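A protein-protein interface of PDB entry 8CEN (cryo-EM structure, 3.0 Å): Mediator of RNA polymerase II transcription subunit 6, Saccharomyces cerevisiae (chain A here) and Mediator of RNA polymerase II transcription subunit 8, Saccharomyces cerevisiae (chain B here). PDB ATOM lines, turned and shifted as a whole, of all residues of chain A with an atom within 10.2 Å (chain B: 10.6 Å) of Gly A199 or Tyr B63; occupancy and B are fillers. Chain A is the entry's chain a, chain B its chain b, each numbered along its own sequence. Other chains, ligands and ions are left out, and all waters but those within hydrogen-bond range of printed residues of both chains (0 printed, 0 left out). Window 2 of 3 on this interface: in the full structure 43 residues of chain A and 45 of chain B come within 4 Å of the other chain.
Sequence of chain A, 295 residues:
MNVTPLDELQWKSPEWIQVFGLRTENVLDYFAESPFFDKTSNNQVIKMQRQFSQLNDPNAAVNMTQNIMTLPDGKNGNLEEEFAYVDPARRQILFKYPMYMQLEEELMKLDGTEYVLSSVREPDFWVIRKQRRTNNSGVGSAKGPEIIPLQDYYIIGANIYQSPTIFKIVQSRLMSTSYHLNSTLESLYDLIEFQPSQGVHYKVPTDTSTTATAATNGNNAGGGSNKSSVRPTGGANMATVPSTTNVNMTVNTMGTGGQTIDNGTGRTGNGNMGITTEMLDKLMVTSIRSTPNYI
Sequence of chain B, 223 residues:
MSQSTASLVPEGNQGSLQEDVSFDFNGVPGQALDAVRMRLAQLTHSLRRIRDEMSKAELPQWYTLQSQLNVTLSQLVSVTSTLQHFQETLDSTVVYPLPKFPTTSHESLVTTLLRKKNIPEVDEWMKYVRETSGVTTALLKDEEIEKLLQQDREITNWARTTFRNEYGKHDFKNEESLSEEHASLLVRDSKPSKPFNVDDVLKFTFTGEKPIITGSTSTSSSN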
ATOM      1  N   LEU A 188      -1.315   2.478 -26.223  1.00  0.00           N
ATOM      2  CA  LEU A 188      -2.708   2.663 -25.827  1.00  0.00           C
ATOM      3  C   LEU A 188      -3.328   3.870 -26.520  1.00  0.00           C
ATOM      4  O   LEU A 188      -4.501   3.829 -26.912  1.00  0.00           O
ATOM      5  CB  LEU A 188      -2.817   2.800 -24.309  1.00  0.00           C
ATOM      6  CG  LEU A 188      -4.226   3.017 -23.746  1.00  0.00           C
ATOM      7  CD1 LEU A 188      -5.189   1.936 -24.213  1.00  0.00           C
ATOM      8  CD2 LEU A 188      -4.190   3.066 -22.233  1.00  0.00           C
ATOM      9  N   TYR A 189      -2.561   4.954 -26.682  1.00  0.00           N
ATOM     10  CA  TYR A 189      -3.081   6.119 -27.387  1.00  0.00           C
ATOM     11  C   TYR A 189      -3.277   5.845 -28.870  1.00  0.00           C
ATOM     12  O   TYR A 189      -4.063   6.544 -29.517  1.00  0.00           O
ATOM     13  CB  TYR A 189      -2.173   7.341 -27.233  1.00  0.00           C
ATOM     14  CG  TYR A 189      -2.128   7.948 -25.849  1.00  0.00           C
ATOM     15  CD1 TYR A 189      -3.286   8.100 -25.094  1.00  0.00           C
ATOM     16  CD2 TYR A 189      -0.919   8.318 -25.272  1.00  0.00           C
ATOM     17  CE1 TYR A 189      -3.241   8.653 -23.826  1.00  0.00           C
ATOM     18  CE2 TYR A 189      -0.866   8.868 -24.007  1.00  0.00           C
ATOM     19  CZ  TYR A 189      -2.028   9.028 -23.287  1.00  0.00           C
ATOM     20  OH  TYR A 189      -1.972   9.569 -22.023  1.00  0.00           O
ATOM     21  N   ILE A 192      -7.028   5.005 -29.463  1.00  0.00           N
ATOM     22  CA  ILE A 192      -7.974   6.025 -29.026  1.00  0.00           C
ATOM     23  C   ILE A 192      -8.569   6.714 -30.245  1.00  0.00           C
ATOM     24  O   ILE A 192      -7.837   7.181 -31.126  1.00  0.00           O
ATOM     25  CB  ILE A 192      -7.302   7.043 -28.088  1.00  0.00           C
ATOM     26  CG1 ILE A 192      -6.740   6.326 -26.865  1.00  0.00           C
ATOM     27  CG2 ILE A 192      -8.280   8.119 -27.666  1.00  0.00           C
ATOM     28  CD1 ILE A 192      -7.798   5.625 -26.055  1.00  0.00           C
ATOM     29  N   GLU A 193      -9.898   6.766 -30.295  1.00  0.00           N
ATOM     30  CA  GLU A 193     -10.635   7.509 -31.303  1.00  0.00           C
ATOM     31  C   GLU A 193     -11.522   8.531 -30.604  1.00  0.00           C
ATOM     32  O   GLU A 193     -12.138   8.236 -29.576  1.00  0.00           O
ATOM     33  CB  GLU A 193     -11.477   6.561 -32.180  1.00  0.00           C
ATOM     34  CG  GLU A 193     -12.529   7.235 -33.050  1.00  0.00           C
ATOM     35  CD  GLU A 193     -13.651   6.296 -33.451  1.00  0.00           C
ATOM     36  OE1 GLU A 193     -14.528   6.018 -32.605  1.00  0.00           O
ATOM     37  OE2 GLU A 193     -13.655   5.834 -34.611  1.00  0.00           O
ATOM     38  N   PHE A 194     -11.584   9.738 -31.160  1.00  0.00           N
ATOM     39  CA  PHE A 194     -12.364  10.820 -30.581  1.00  0.00           C
ATOM     40  C   PHE A 194     -13.592  11.109 -31.430  1.00  0.00           C
ATOM     41  O   PHE A 194     -13.507  11.187 -32.660  1.00  0.00           O
ATOM     42  CB  PHE A 194     -11.530  12.097 -30.435  1.00  0.00           C
ATOM     43  CG  PHE A 194     -12.339  13.303 -30.046  1.00  0.00           C
ATOM     44  CD1 PHE A 194     -12.871  13.415 -28.770  1.00  0.00           C
ATOM     45  CD2 PHE A 194     -12.570  14.322 -30.955  1.00  0.00           C
ATOM     46  CE1 PHE A 194     -13.621  14.519 -28.412  1.00  0.00           C
ATOM     47  CE2 PHE A 194     -13.317  15.429 -30.603  1.00  0.00           C
ATOM     48  CZ  PHE A 194     -13.843  15.529 -29.329  1.00  0.00           C
ATOM     49  N   GLN A 195     -14.731  11.267 -30.761  1.00  0.00           N
ATOM     50  CA  GLN A 195     -15.987  11.639 -31.382  1.00  0.00           C
ATOM     51  C   GLN A 195     -16.603  12.794 -30.606  1.00  0.00           C
ATOM     52  O   GLN A 195     -16.484  12.847 -29.377  1.00  0.00           O
ATOM     53  CB  GLN A 195     -16.962  10.454 -31.413  1.00  0.00           C
ATOM     54  CG  GLN A 195     -16.907   9.628 -32.686  1.00  0.00           C
ATOM     55  CD  GLN A 195     -18.042   8.626 -32.777  1.00  0.00           C
ATOM     56  OE1 GLN A 195     -19.107   8.822 -32.191  1.00  0.00           O
ATOM     57  NE2 GLN A 195     -17.818   7.544 -33.513  1.00  0.00           N
ATOM     58  N   PRO A 196     -17.242  13.737 -31.287  1.00  0.00           N
ATOM     59  CA  PRO A 196     -17.904  14.836 -30.574  1.00  0.00           C
ATOM     60  C   PRO A 196     -19.287  14.442 -30.082  1.00  0.00           C
ATOM     61  O   PRO A 196     -19.772  14.970 -29.076  1.00  0.00           O
ATOM     62  CB  PRO A 196     -17.977  15.947 -31.633  1.00  0.00           C
ATOM     63  CG  PRO A 196     -17.010  15.516 -32.715  1.00  0.00           C
ATOM     64  CD  PRO A 196     -17.103  14.033 -32.718  1.00  0.00           C
ATOM     65  N   SER A 197     -19.924  13.502 -30.787  1.00  0.00           N
ATOM     66  CA  SER A 197     -21.259  13.046 -30.414  1.00  0.00           C
ATOM     67  C   SER A 197     -21.255  12.236 -29.126  1.00  0.00           C
ATOM     68  O   SER A 197     -22.293  12.140 -28.462  1.00  0.00           O
ATOM     69  CB  SER A 197     -21.869  12.221 -31.548  1.00  0.00           C
ATOM     70  OG  SER A 197     -21.043  11.120 -31.881  1.00  0.00           O
ATOM     71  N   GLN A 198     -20.121  11.654 -28.767  1.00  0.00           N
ATOM     72  CA  GLN A 198     -19.928  10.927 -27.524  1.00  0.00           C
ATOM     73  C   GLN A 198     -18.726  11.531 -26.803  1.00  0.00           C
ATOM     74  O   GLN A 198     -18.233  12.602 -27.166  1.00  0.00           O
ATOM     75  CB  GLN A 198     -19.737   9.433 -27.795  1.00  0.00           C
ATOM     76  CG  GLN A 198     -20.863   8.789 -28.590  1.00  0.00           C
ATOM     77  CD  GLN A 198     -20.410   7.559 -29.350  1.00  0.00           C
ATOM     78  OE1 GLN A 198     -19.214   7.293 -29.469  1.00  0.00           O
ATOM     79  NE2 GLN A 198     -21.367   6.799 -29.870  1.00  0.00           N
ATOM     80  N   GLY A 199     -18.271  10.854 -25.755  1.00  0.00           N
ATOM     81  CA  GLY A 199     -16.987  11.171 -25.173  1.00  0.00           C
ATOM     82  C   GLY A 199     -15.864  10.540 -25.970  1.00  0.00           C
ATOM     83  O   GLY A 199     -16.076   9.813 -26.941  1.00  0.00           O
ATOM     84  N   VAL A 200     -14.634  10.834 -25.552  1.00  0.00           N
ATOM     85  CA  VAL A 200     -13.484  10.158 -26.135  1.00  0.00           C
ATOM     86  C   VAL A 200     -13.446   8.721 -25.624  1.00  0.00           C
ATOM     87  O   VAL A 200     -13.687   8.454 -24.439  1.00  0.00           O
ATOM     88  CB  VAL A 200     -12.191  10.946 -25.853  1.00  0.00           C
ATOM     89  CG1 VAL A 200     -11.866  11.019 -24.366  1.00  0.00           C
ATOM     90  CG2 VAL A 200     -11.027  10.357 -26.629  1.00  0.00           C
ATOM     91  N   HIS A 201     -13.222   7.778 -26.534  1.00  0.00           N
ATOM     92  CA  HIS A 201     -13.417   6.366 -26.227  1.00  0.00           C
ATOM     93  C   HIS A 201     -12.464   5.535 -27.079  1.00  0.00           C
ATOM     94  O   HIS A 201     -11.550   6.062 -27.719  1.00  0.00           O
ATOM     95  CB  HIS A 201     -14.884   5.975 -26.446  1.00  0.00           C
ATOM     96  CG  HIS A 201     -15.346   6.142 -27.860  1.00  0.00           C
ATOM     97  ND1 HIS A 201     -15.634   7.373 -28.408  1.00  0.00           N
ATOM     98  CD2 HIS A 201     -15.570   5.234 -28.839  1.00  0.00           C
ATOM     99  CE1 HIS A 201     -16.013   7.217 -29.664  1.00  0.00           C
ATOM    100  NE2 HIS A 201     -15.984   5.927 -29.950  1.00  0.00           N
ATOM    101  N   TYR A 202     -12.689   4.223 -27.087  1.00  0.00           N
ATOM    102  CA  TYR A 202     -11.815   3.284 -27.775  1.00  0.00           C
ATOM    103  C   TYR A 202     -12.306   3.037 -29.193  1.00  0.00           C
ATOM    104  O   TYR A 202     -13.512   2.991 -29.447  1.00  0.00           O
ATOM    105  CB  TYR A 202     -11.741   1.957 -27.020  1.00  0.00           C
ATOM    106  CG  TYR A 202     -11.303   2.094 -25.583  1.00  0.00           C
ATOM    107  CD1 TYR A 202      -9.956   2.099 -25.246  1.00  0.00           C
ATOM    108  CD2 TYR A 202     -12.237   2.214 -24.564  1.00  0.00           C
ATOM    109  CE1 TYR A 202      -9.552   2.223 -23.932  1.00  0.00           C
ATOM    110  CE2 TYR A 202     -11.843   2.340 -23.250  1.00  0.00           C
ATOM    111  CZ  TYR A 202     -10.500   2.343 -22.939  1.00  0.00           C
ATOM    112  OH  TYR A 202     -10.104   2.467 -21.628  1.00  0.00           O
ATOM    113  N   LYS A 203     -11.358   2.873 -30.111  1.00  0.00           N
ATOM    114  CA  LYS A 203     -11.690   2.598 -31.502  1.00  0.00           C
ATOM    115  C   LYS A 203     -12.288   1.201 -31.633  1.00  0.00           C
ATOM    116  O   LYS A 203     -11.752   0.229 -31.092  1.00  0.00           O
ATOM    117  CB  LYS A 203     -10.443   2.730 -32.371  1.00  0.00           C
ATOM    118  CG  LYS A 203     -10.710   3.175 -33.800  1.00  0.00           C
ATOM    119  CD  LYS A 203      -9.414   3.509 -34.528  1.00  0.00           C
ATOM    120  CE  LYS A 203      -8.515   4.417 -33.701  1.00  0.00           C
ATOM    121  NZ  LYS A 203      -7.182   4.606 -34.334  1.00  0.00           N
ATOM    122  N   GLU B  53      -6.300  -4.649 -14.171  1.00  0.00           N
ATOM    123  CA  GLU B  53      -7.496  -4.024 -14.714  1.00  0.00           C
ATOM    124  C   GLU B  53      -7.492  -4.010 -16.236  1.00  0.00           C
ATOM    125  O   GLU B  53      -8.557  -4.075 -16.857  1.00  0.00           O
ATOM    126  CB  GLU B  53      -7.611  -2.590 -14.173  1.00  0.00           C
ATOM    127  CG  GLU B  53      -8.752  -1.722 -14.705  1.00  0.00           C
ATOM    128  CD  GLU B  53     -10.132  -2.300 -14.418  1.00  0.00           C
ATOM    129  OE1 GLU B  53     -10.728  -1.915 -13.390  1.00  0.00           O
ATOM    130  OE2 GLU B  53     -10.636  -3.115 -15.218  1.00  0.00           O
ATOM    131  N   LEU B  59     -11.886  -3.620 -21.899  1.00  0.00           N
ATOM    132  CA  LEU B  59     -11.141  -2.506 -21.336  1.00  0.00           C
ATOM    133  C   LEU B  59     -12.000  -1.738 -20.333  1.00  0.00           C
ATOM    134  O   LEU B  59     -13.224  -1.673 -20.473  1.00  0.00           O
ATOM    135  CB  LEU B  59     -10.672  -1.554 -22.437  1.00  0.00           C
ATOM    136  CG  LEU B  59      -9.379  -1.824 -23.217  1.00  0.00           C
ATOM    137  CD1 LEU B  59      -8.171  -1.791 -22.284  1.00  0.00           C
ATOM    138  CD2 LEU B  59      -9.420  -3.118 -24.021  1.00  0.00           C
ATOM    139  N   PRO B  60     -11.384  -1.145 -19.313  1.00  0.00           N
ATOM    140  CA  PRO B  60     -12.124  -0.244 -18.424  1.00  0.00           C
ATOM    141  C   PRO B  60     -12.499   1.041 -19.144  1.00  0.00           C
ATOM    142  O   PRO B  60     -12.064   1.312 -20.266  1.00  0.00           O
ATOM    143  CB  PRO B  60     -11.138   0.017 -17.283  1.00  0.00           C
ATOM    144  CG  PRO B  60      -9.800  -0.191 -17.906  1.00  0.00           C
ATOM    145  CD  PRO B  60      -9.994  -1.333 -18.861  1.00  0.00           C
ATOM    146  N   GLN B  61     -13.342   1.833 -18.482  1.00  0.00           N
ATOM    147  CA  GLN B  61     -13.753   3.115 -19.040  1.00  0.00           C
ATOM    148  C   GLN B  61     -12.547   4.039 -19.164  1.00  0.00           C
ATOM    149  O   GLN B  61     -11.689   4.086 -18.277  1.00  0.00           O
ATOM    150  CB  GLN B  61     -14.836   3.751 -18.167  1.00  0.00           C
ATOM    151  CG  GLN B  61     -15.388   5.058 -18.712  1.00  0.00           C
ATOM    152  CD  GLN B  61     -16.063   4.883 -20.060  1.00  0.00           C
ATOM    153  OE1 GLN B  61     -15.510   5.251 -21.097  1.00  0.00           O
ATOM    154  NE2 GLN B  61     -17.263   4.313 -20.052  1.00  0.00           N
ATOM    155  N   TRP B  62     -12.479   4.757 -20.290  1.00  0.00           N
ATOM    156  CA  TRP B  62     -11.259   5.469 -20.653  1.00  0.00           C
ATOM    157  C   TRP B  62     -10.953   6.620 -19.704  1.00  0.00           C
ATOM    158  O   TRP B  62      -9.780   6.918 -19.470  1.00  0.00           O
ATOM    159  CB  TRP B  62     -11.344   5.962 -22.100  1.00  0.00           C
ATOM    160  CG  TRP B  62     -10.315   6.991 -22.432  1.00  0.00           C
ATOM    161  CD1 TRP B  62     -10.519   8.325 -22.612  1.00  0.00           C
ATOM    162  CD2 TRP B  62      -8.902   6.783 -22.546  1.00  0.00           C
ATOM    163  NE1 TRP B  62      -9.327   8.957 -22.876  1.00  0.00           N
ATOM    164  CE2 TRP B  62      -8.318   8.031 -22.835  1.00  0.00           C
ATOM    165  CE3 TRP B  62      -8.078   5.658 -22.447  1.00  0.00           C
ATOM    166  CZ2 TRP B  62      -6.950   8.187 -23.028  1.00  0.00           C
ATOM    167  CZ3 TRP B  62      -6.719   5.815 -22.638  1.00  0.00           C
ATOM    168  CH2 TRP B  62      -6.169   7.069 -22.925  1.00  0.00           C
ATOM    169  N   TYR B  63     -11.979   7.260 -19.133  1.00  0.00           N
ATOM    170  CA  TYR B  63     -11.732   8.301 -18.137  1.00  0.00           C
ATOM    171  C   TYR B  63     -11.046   7.731 -16.899  1.00  0.00           C
ATOM    172  O   TYR B  63     -10.068   8.304 -16.401  1.00  0.00           O
ATOM    173  CB  TYR B  63     -13.044   8.987 -17.755  1.00  0.00           C
ATOM    174  CG  TYR B  63     -13.638   9.858 -18.840  1.00  0.00           C
ATOM    175  CD1 TYR B  63     -12.857  10.328 -19.890  1.00  0.00           C
ATOM    176  CD2 TYR B  63     -14.982  10.212 -18.814  1.00  0.00           C
ATOM    177  CE1 TYR B  63     -13.399  11.125 -20.884  1.00  0.00           C
ATOM    178  CE2 TYR B  63     -15.533  11.008 -19.802  1.00  0.00           C
ATOM    179  CZ  TYR B  63     -14.737  11.462 -20.834  1.00  0.00           C
ATOM    180  OH  TYR B  63     -15.281  12.254 -21.819  1.00  0.00           O
ATOM    181  N   THR B  64     -11.530   6.584 -16.410  1.00  0.00           N
ATOM    182  CA  THR B  64     -10.908   5.934 -15.261  1.00  0.00           C
ATOM    183  C   THR B  64      -9.501   5.447 -15.587  1.00  0.00           C
ATOM    184  O   THR B  64      -8.585   5.583 -14.765  1.00  0.00           O
ATOM    185  CB  THR B  64     -11.772   4.767 -14.786  1.00  0.00           C
ATOM    186  OG1 THR B  64     -12.258   4.038 -15.921  1.00  0.00           O
ATOM    187  CG2 THR B  64     -12.953   5.275 -13.972  1.00  0.00           C
ATOM    188  N   LEU B  65      -9.312   4.879 -16.782  1.00  0.00           N
ATOM    189  CA  LEU B  65      -7.992   4.403 -17.182  1.00  0.00           C
ATOM    190  C   LEU B  65      -7.001   5.553 -17.314  1.00  0.00           C
ATOM    191  O   LEU B  65      -5.845   5.432 -16.893  1.00  0.00           O
ATOM    192  CB  LEU B  65      -8.087   3.625 -18.495  1.00  0.00           C
ATOM    193  CG  LEU B  65      -6.829   2.880 -18.948  1.00  0.00           C
ATOM    194  CD1 LEU B  65      -6.202   2.107 -17.797  1.00  0.00           C
ATOM    195  CD2 LEU B  65      -7.144   1.953 -20.110  1.00  0.00           C
ATOM    196  N   GLN B  66      -7.440   6.682 -17.879  1.00  0.00           N
ATOM    197  CA  GLN B  66      -6.578   7.850 -17.998  1.00  0.00           C
ATOM    198  C   GLN B  66      -6.257   8.442 -16.634  1.00  0.00           C
ATOM    199  O   GLN B  66      -5.138   8.915 -16.409  1.00  0.00           O
ATOM    200  CB  GLN B  66      -7.235   8.896 -18.899  1.00  0.00           C
ATOM    201  CG  GLN B  66      -6.380  10.123 -19.166  1.00  0.00           C
ATOM    202  CD  GLN B  66      -7.047  11.103 -20.106  1.00  0.00           C
ATOM    203  OE1 GLN B  66      -8.179  10.890 -20.543  1.00  0.00           O
ATOM    204  NE2 GLN B  66      -6.348  12.186 -20.427  1.00  0.00           N
ATOM    205  N   SER B  67      -7.221   8.421 -15.706  1.00  0.00           N
ATOM    206  CA  SER B  67      -6.942   8.885 -14.351  1.00  0.00           C
ATOM    207  C   SER B  67      -5.911   7.996 -13.663  1.00  0.00           C
ATOM    208  O   SER B  67      -4.996   8.498 -12.999  1.00  0.00           O
ATOM    209  CB  SER B  67      -8.234   8.940 -13.536  1.00  0.00           C
ATOM    210  OG  SER B  67      -8.768   7.644 -13.339  1.00  0.00           O
ATOM    211  N   GLN B  68      -6.032   6.674 -13.831  1.00  0.00           N
ATOM    212  CA  GLN B  68      -5.046   5.755 -13.266  1.00  0.00           C
ATOM    213  C   GLN B  68      -3.668   5.963 -13.885  1.00  0.00           C
ATOM    214  O   GLN B  68      -2.652   5.929 -13.179  1.00  0.00           O
ATOM    215  CB  GLN B  68      -5.502   4.308 -13.457  1.00  0.00           C
ATOM    216  CG  GLN B  68      -6.741   3.928 -12.666  1.00  0.00           C
ATOM    217  CD  GLN B  68      -7.164   2.493 -12.905  1.00  0.00           C
ATOM    218  OE1 GLN B  68      -6.567   1.786 -13.717  1.00  0.00           O
ATOM    219  NE2 GLN B  68      -8.195   2.052 -12.193  1.00  0.00           N
ATOM    220  N   LEU B  69      -3.617   6.183 -15.202  1.00  0.00           N
ATOM    221  CA  LEU B  69      -2.347   6.446 -15.872  1.00  0.00           C
ATOM    222  C   LEU B  69      -1.721   7.751 -15.394  1.00  0.00           C
ATOM    223  O   LEU B  69      -0.502   7.829 -15.216  1.00  0.00           O
ATOM    224  CB  LEU B  69      -2.552   6.475 -17.385  1.00  0.00           C
ATOM    225  CG  LEU B  69      -2.828   5.132 -18.059  1.00  0.00           C
ATOM    226  CD1 LEU B  69      -3.255   5.352 -19.494  1.00  0.00           C
ATOM    227  CD2 LEU B  69      -1.608   4.232 -17.993  1.00  0.00           C
ATOM    228  N   ASN B  70      -2.542   8.785 -15.178  1.00  0.00           N
ATOM    229  CA  ASN B  70      -2.025  10.054 -14.676  1.00  0.00           C
ATOM    230  C   ASN B  70      -1.500   9.920 -13.251  1.00  0.00           C
ATOM    231  O   ASN B  70      -0.471  10.516 -12.912  1.00  0.00           O
ATOM    232  CB  ASN B  70      -3.104  11.134 -14.751  1.00  0.00           C
ATOM    233  CG  ASN B  70      -3.456  11.506 -16.178  1.00  0.00           C
ATOM    234  OD1 ASN B  70      -2.605  11.471 -17.067  1.00  0.00           O
ATOM    235  ND2 ASN B  70      -4.714  11.867 -16.405  1.00  0.00           N
ATOM    236  N   VAL B  71      -2.191   9.148 -12.406  1.00  0.00           N
ATOM    237  CA  VAL B  71      -1.694   8.899 -11.051  1.00  0.00           C
ATOM    238  C   VAL B  71      -0.378   8.129 -11.091  1.00  0.00           C
ATOM    239  O   VAL B  71       0.556   8.431 -10.339  1.00  0.00           O
ATOM    240  CB  VAL B  71      -2.763   8.175 -10.207  1.00  0.00           C
ATOM    241  CG1 VAL B  71      -2.216   7.812  -8.838  1.00  0.00           C
ATOM    242  CG2 VAL B  71      -3.972   9.069 -10.022  1.00  0.00           C
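The side-chain hydroxyl (OH) of Tyr A202 lies within hydrogen-bond range of the backbone carbonyl oxygen (O) of Pro B60 (2.7 Å).
Of the 14 printed residues of chain A, 6 touch a printed residue of chain B. Printed residues of chain A that touch a printed residue of chain B: Leu A188, Tyr A189, Ile A192, Gly A199, Val A200 and Tyr A202. Hydrophobic or aromatic side chains of chain A within 4 Å of the printed part of chain B: Leu A188, Tyr A189, Ile A192, Val A200 and Tyr A202. Of the 14 printed residues of chain B, 7 touch a printed residue of chain A. Printed residues of chain B that touch a printed residue of chain A: Leu B59, Pro B60, Gln B61, Trp B62, Tyr B63, Leu B65 and Leu B69.
Trp B62 touches Leu A188. Leu B65 touches Leu A188 (CD2 to CD2, 3.8 Å). CD2 of Leu A188 touches CD1 of Leu B69, at 3.7 Å. Trp B62 touches Tyr A189. Ile A192 touches Trp B62. Gly A199 touches Tyr B63. Leu B59 touches Tyr A202. Gln B61 touches Tyr A202. Trp B62 touches Tyr A202. Leu B65 touches Tyr A202 (CD2 to OH, 3.4 Å).
O of Tyr B63 is in hydrogen-bond range of OG of Ser B67. The backbone carbonyl oxygen of Gln B61 sits at hydrogen-bond distance from the side-chain hydroxyl of Thr B64 (2.4 Å). ND1 of His A201 lies within hydrogen-bond range of O of Gly A199. The indole nitrogen of Trp B62 lies within hydrogen-bond range of the side-chain amide oxygen of Gln B66 (3.2 Å).
Ser A197 touches none of the printed residues of chain B. Gly A199 touches one residue of chain B. Of chain B, only Trp B62 (3.5 Å) and Tyr B63 (3.8 Å) come within 4 Å of Val A200. No residue of chain B comes within 4 Å of His A201. Of the printed residues of chain A, Leu B59 touches Tyr A202 (3.9 Å). No residue of chain A comes within 4 Å of Thr B64. Of the printed residues of chain A, Leu B65 touches Leu A188 and Tyr A202. No residue of chain A comes within 4 Å of Ser B67. The nearest residue of chain B that does not touch Gly A199 is Trp B62 (6.7 Å). The nearest printed residue of chain A that does not touch Leu B65 is Ile A192 (7.0 Å).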
